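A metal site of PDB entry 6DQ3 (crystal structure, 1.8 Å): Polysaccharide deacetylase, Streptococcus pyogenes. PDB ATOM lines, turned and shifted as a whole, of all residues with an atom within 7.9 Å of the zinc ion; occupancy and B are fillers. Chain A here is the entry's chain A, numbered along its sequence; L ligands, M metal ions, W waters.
OD1 of Asp 78 binds the zinc ion (2.1 Å). The zinc ion is bound by NE2 of His 137 (2.1 Å). The zinc ion is bound by NE2 of His 133 (2.2 Å). An oxygen (O2) of the ligand is bound to the zinc ion, 2.2 Å away. Water W1 binds the zinc ion, at 2.4 Å. O1 of the ligand binds the zinc ion. The zinc ion has six donor atoms within binding distance.
Of the 18 residues printed, 3 come within 4 Å of the zinc ion. The nearest printed residue that does not touch the zinc ion is Asp 77 (4.3 Å).
The backbone NH of Asp 78 sits at hydrogen-bond distance from the backbone carbonyl oxygen of Asn 101, 3.0 Å away. N of His 137 lies within hydrogen-bond range of OG1 of Thr 134 (2.8 Å). O of Ala 171 sits at hydrogen-bond distance from ND1 of His 133 (2.6 Å).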
ATOM      1  N   HIS A  15       3.669  21.396  -9.526  1.00  0.00           N
ATOM      2  CA  HIS A  15       4.022  22.554  -8.723  1.00  0.00           C
ATOM      3  C   HIS A  15       4.579  23.604  -9.670  1.00  0.00           C
ATOM      4  O   HIS A  15       3.808  24.300 -10.346  1.00  0.00           O
ATOM      5  CB  HIS A  15       5.004  22.178  -7.609  1.00  0.00           C
ATOM      6  CG  HIS A  15       4.312  21.602  -6.402  1.00  0.00           C
ATOM      7  ND1 HIS A  15       3.860  20.306  -6.355  1.00  0.00           N
ATOM      8  CD2 HIS A  15       4.001  22.165  -5.211  1.00  0.00           C
ATOM      9  CE1 HIS A  15       3.299  20.079  -5.179  1.00  0.00           C
ATOM     10  NE2 HIS A  15       3.380  21.188  -4.463  1.00  0.00           N
ATOM     11  N   PHE A  76      -2.577  21.862  -9.245  1.00  0.00           N
ATOM     12  CA  PHE A  76      -1.364  22.640  -9.010  1.00  0.00           C
ATOM     13  C   PHE A  76      -1.458  23.226  -7.603  1.00  0.00           C
ATOM     14  O   PHE A  76      -2.454  23.880  -7.269  1.00  0.00           O
ATOM     15  CB  PHE A  76      -1.233  23.794 -10.011  1.00  0.00           C
ATOM     16  CG  PHE A  76      -0.927  23.365 -11.414  1.00  0.00           C
ATOM     17  CD1 PHE A  76      -1.874  22.700 -12.184  1.00  0.00           C
ATOM     18  CD2 PHE A  76       0.303  23.656 -11.995  1.00  0.00           C
ATOM     19  CE1 PHE A  76      -1.599  22.313 -13.476  1.00  0.00           C
ATOM     20  CE2 PHE A  76       0.583  23.274 -13.294  1.00  0.00           C
ATOM     21  CZ  PHE A  76      -0.367  22.602 -14.028  1.00  0.00           C
ATOM     22  N   ASP A  77      -0.423  23.035  -6.794  1.00  0.00           N
ATOM     23  CA  ASP A  77      -0.426  23.591  -5.451  1.00  0.00           C
ATOM     24  C   ASP A  77       0.356  24.908  -5.381  1.00  0.00           C
ATOM     25  O   ASP A  77       1.203  25.199  -6.223  1.00  0.00           O
ATOM     26  CB  ASP A  77       0.184  22.596  -4.442  1.00  0.00           C
ATOM     27  CG  ASP A  77      -0.539  21.271  -4.409  1.00  0.00           C
ATOM     28  OD1 ASP A  77      -1.728  21.216  -4.797  1.00  0.00           O
ATOM     29  OD2 ASP A  77       0.067  20.268  -3.988  1.00  0.00           O
ATOM     30  N   ASP A  78       0.002  25.702  -4.367  1.00  0.00           N
ATOM     31  CA  ASP A  78       0.779  26.836  -3.860  1.00  0.00           C
ATOM     32  C   ASP A  78       0.542  28.148  -4.611  1.00  0.00           C
ATOM     33  O   ASP A  78       1.189  29.162  -4.323  1.00  0.00           O
ATOM     34  CB  ASP A  78       2.276  26.493  -3.873  1.00  0.00           C
ATOM     35  CG  ASP A  78       2.647  25.416  -2.868  1.00  0.00           C
ATOM     36  OD1 ASP A  78       1.794  25.091  -2.028  1.00  0.00           O
ATOM     37  OD2 ASP A  78       3.781  24.885  -2.935  1.00  0.00           O
ATOM     38  N   SER A  79      -0.410  28.136  -5.535  1.00  0.00           N
ATOM     39  CA  SER A  79      -0.877  29.338  -6.237  1.00  0.00           C
ATOM     40  C   SER A  79       0.282  30.259  -6.608  1.00  0.00           C
ATOM     41  O   SER A  79       0.300  31.449  -6.295  1.00  0.00           O
ATOM     42  CB  SER A  79      -1.921  30.071  -5.391  1.00  0.00           C
ATOM     43  OG  SER A  79      -1.521  30.176  -4.032  1.00  0.00           O
ATOM     44  N   ASN A 101      -4.608  25.001  -6.011  1.00  0.00           N
ATOM     45  CA  ASN A 101      -4.892  25.038  -4.581  1.00  0.00           C
ATOM     46  C   ASN A 101      -4.177  26.224  -3.961  1.00  0.00           C
ATOM     47  O   ASN A 101      -2.944  26.263  -3.924  1.00  0.00           O
ATOM     48  CB  ASN A 101      -4.494  23.705  -3.968  1.00  0.00           C
ATOM     49  CG  ASN A 101      -5.227  22.547  -4.635  1.00  0.00           C
ATOM     50  OD1 ASN A 101      -6.449  22.586  -4.761  1.00  0.00           O
ATOM     51  ND2 ASN A 101      -4.493  21.545  -5.094  1.00  0.00           N
ATOM     52  N   ILE A 103      -2.993  29.352  -1.510  1.00  0.00           N
ATOM     53  CA  ILE A 103      -2.567  29.830  -0.203  1.00  0.00           C
ATOM     54  C   ILE A 103      -3.125  31.245  -0.064  1.00  0.00           C
ATOM     55  O   ILE A 103      -2.543  32.200  -0.584  1.00  0.00           O
ATOM     56  CB  ILE A 103      -1.042  29.809  -0.051  1.00  0.00           C
ATOM     57  CG1 ILE A 103      -0.497  28.416  -0.365  1.00  0.00           C
ATOM     58  CG2 ILE A 103      -0.632  30.262   1.341  1.00  0.00           C
ATOM     59  CD1 ILE A 103       1.016  28.355  -0.477  1.00  0.00           C
ATOM     60  N   HIS A 133      -5.838  25.833  -0.028  1.00  0.00           N
ATOM     61  CA  HIS A 133      -4.528  25.377   0.417  1.00  0.00           C
ATOM     62  C   HIS A 133      -4.127  26.089   1.703  1.00  0.00           C
ATOM     63  O   HIS A 133      -2.943  26.357   1.926  1.00  0.00           O
ATOM     64  CB  HIS A 133      -3.495  25.573  -0.689  1.00  0.00           C
ATOM     65  CG  HIS A 133      -2.315  24.657  -0.594  1.00  0.00           C
ATOM     66  ND1 HIS A 133      -2.406  23.361  -0.128  1.00  0.00           N
ATOM     67  CD2 HIS A 133      -1.021  24.844  -0.943  1.00  0.00           C
ATOM     68  CE1 HIS A 133      -1.211  22.789  -0.172  1.00  0.00           C
ATOM     69  NE2 HIS A 133      -0.345  23.671  -0.663  1.00  0.00           N
ATOM     70  N   THR A 134      -5.123  26.385   2.557  1.00  0.00           N
ATOM     71  CA  THR A 134      -4.991  27.055   3.849  1.00  0.00           C
ATOM     72  C   THR A 134      -4.640  28.531   3.705  1.00  0.00           C
ATOM     73  O   THR A 134      -4.355  29.013   2.601  1.00  0.00           O
ATOM     74  CB  THR A 134      -3.945  26.395   4.760  1.00  0.00           C
ATOM     75  OG1 THR A 134      -2.631  26.791   4.372  1.00  0.00           O
ATOM     76  CG2 THR A 134      -4.066  24.868   4.746  1.00  0.00           C
ATOM     77  N   HIS A 137      -0.364  28.168   5.140  1.00  0.00           N
ATOM     78  CA  HIS A 137       0.394  26.983   4.754  1.00  0.00           C
ATOM     79  C   HIS A 137       1.160  26.382   5.939  1.00  0.00           C
ATOM     80  O   HIS A 137       2.346  26.038   5.795  1.00  0.00           O
ATOM     81  CB  HIS A 137       1.364  27.331   3.625  1.00  0.00           C
ATOM     82  CG  HIS A 137       1.753  26.172   2.751  1.00  0.00           C
ATOM     83  ND1 HIS A 137       2.882  25.417   2.978  1.00  0.00           N
ATOM     84  CD2 HIS A 137       1.171  25.671   1.636  1.00  0.00           C
ATOM     85  CE1 HIS A 137       2.977  24.481   2.041  1.00  0.00           C
ATOM     86  NE2 HIS A 137       1.952  24.612   1.221  1.00  0.00           N
ATOM     87  N   PRO A 138       0.517  26.217   7.095  1.00  0.00           N
ATOM     88  CA  PRO A 138       1.168  25.481   8.188  1.00  0.00           C
ATOM     89  C   PRO A 138       1.143  23.978   7.943  1.00  0.00           C
ATOM     90  O   PRO A 138       0.407  23.462   7.099  1.00  0.00           O
ATOM     91  CB  PRO A 138       0.311  25.849   9.399  1.00  0.00           C
ATOM     92  CG  PRO A 138      -1.075  25.960   8.812  1.00  0.00           C
ATOM     93  CD  PRO A 138      -0.851  26.623   7.452  1.00  0.00           C
ATOM     94  N   ALA A 171      -6.165  20.897  -0.501  1.00  0.00           N
ATOM     95  CA  ALA A 171      -4.895  20.171  -0.529  1.00  0.00           C
ATOM     96  C   ALA A 171      -4.161  20.490   0.773  1.00  0.00           C
ATOM     97  O   ALA A 171      -3.935  21.663   1.080  1.00  0.00           O
ATOM     98  CB  ALA A 171      -4.050  20.573  -1.740  1.00  0.00           C
ATOM     99  N   TYR A 172      -3.803  19.456   1.532  1.00  0.00           N
ATOM    100  CA  TYR A 172      -3.130  19.688   2.811  1.00  0.00           C
ATOM    101  C   TYR A 172      -1.680  20.090   2.572  1.00  0.00           C
ATOM    102  O   TYR A 172      -0.996  19.446   1.774  1.00  0.00           O
ATOM    103  CB  TYR A 172      -3.201  18.424   3.682  1.00  0.00           C
ATOM    104  CG  TYR A 172      -4.609  17.910   3.778  1.00  0.00           C
ATOM    105  CD1 TYR A 172      -5.604  18.663   4.373  1.00  0.00           C
ATOM    106  CD2 TYR A 172      -4.960  16.681   3.234  1.00  0.00           C
ATOM    107  CE1 TYR A 172      -6.895  18.213   4.437  1.00  0.00           C
ATOM    108  CE2 TYR A 172      -6.250  16.220   3.290  1.00  0.00           C
ATOM    109  CZ  TYR A 172      -7.219  16.998   3.893  1.00  0.00           C
ATOM    110  OH  TYR A 172      -8.511  16.548   3.957  1.00  0.00           O
ATOM    111  N   PRO A 173      -1.187  21.136   3.225  1.00  0.00           N
ATOM    112  CA  PRO A 173       0.204  21.547   3.012  1.00  0.00           C
ATOM    113  C   PRO A 173       1.169  20.407   3.304  1.00  0.00           C
ATOM    114  O   PRO A 173       1.131  19.779   4.372  1.00  0.00           O
ATOM    115  CB  PRO A 173       0.391  22.720   3.973  1.00  0.00           C
ATOM    116  CG  PRO A 173      -0.983  23.322   4.050  1.00  0.00           C
ATOM    117  CD  PRO A 173      -1.932  22.131   4.026  1.00  0.00           C
ATOM    118  N   SER A 174       2.043  20.142   2.338  1.00  0.00           N
ATOM    119  CA  SER A 174       3.053  19.087   2.413  1.00  0.00           C
ATOM    120  C   SER A 174       2.445  17.706   2.578  1.00  0.00           C
ATOM    121  O   SER A 174       3.146  16.749   2.925  1.00  0.00           O
ATOM    122  CB  SER A 174       4.046  19.387   3.543  1.00  0.00           C
ATOM    123  OG  SER A 174       4.719  20.602   3.294  1.00  0.00           O
ATOM    124  N   GLY A 175       1.147  17.571   2.298  1.00  0.00           N
ATOM    125  CA  GLY A 175       0.483  16.296   2.408  1.00  0.00           C
ATOM    126  C   GLY A 175       0.298  15.795   3.817  1.00  0.00           C
ATOM    127  O   GLY A 175       0.016  14.610   4.002  1.00  0.00           O
ATOM    128  N   THR A 196      -0.308  13.902  -0.657  1.00  0.00           N
ATOM    129  CA  THR A 196       0.842  13.603  -1.499  1.00  0.00           C
ATOM    130  C   THR A 196       1.166  12.112  -1.536  1.00  0.00           C
ATOM    131  O   THR A 196       2.263  11.727  -1.968  1.00  0.00           O
ATOM    132  CB  THR A 196       2.078  14.409  -1.058  1.00  0.00           C
ATOM    133  OG1 THR A 196       2.420  14.101   0.303  1.00  0.00           O
ATOM    134  CG2 THR A 196       1.808  15.915  -1.186  1.00  0.00           C
ATOM    135  N   ARG A 212      -2.468  11.242  -5.098  1.00  0.00           N
ATOM    136  CA  ARG A 212      -2.103  12.013  -6.282  1.00  0.00           C
ATOM    137  C   ARG A 212      -0.851  11.423  -6.926  1.00  0.00           C
ATOM    138  O   ARG A 212      -0.094  10.690  -6.287  1.00  0.00           O
ATOM    139  CB  ARG A 212      -1.876  13.495  -5.937  1.00  0.00           C
ATOM    140  CG  ARG A 212      -3.147  14.223  -5.554  1.00  0.00           C
ATOM    141  CD  ARG A 212      -3.000  15.734  -5.678  1.00  0.00           C
ATOM    142  NE  ARG A 212      -2.267  16.314  -4.561  1.00  0.00           N
ATOM    143  CZ  ARG A 212      -1.953  17.598  -4.451  1.00  0.00           C
ATOM    144  NH1 ARG A 212      -2.313  18.453  -5.405  1.00  0.00           N
ATOM    145  NH2 ARG A 212      -1.285  18.034  -3.388  1.00  0.00           N
HETATM  146  C1  LIG L   1       1.953  21.072  -1.017  1.00  0.00           C
HETATM  147  O1  LIG L   1       2.181  21.730  -2.051  1.00  0.00           O
HETATM  148  O2  LIG L   1       1.968  21.509   0.148  1.00  0.00           O
HETATM  149  C2  LIG L   1       1.631  19.675  -1.203  1.00  0.00           C
HETATM  150 ZN    ZN M   1       1.829  23.612  -0.586  1.00  0.00          ZN
HETATM  151  O   HOH W   1       4.199  23.506  -0.729  1.00  0.00           O
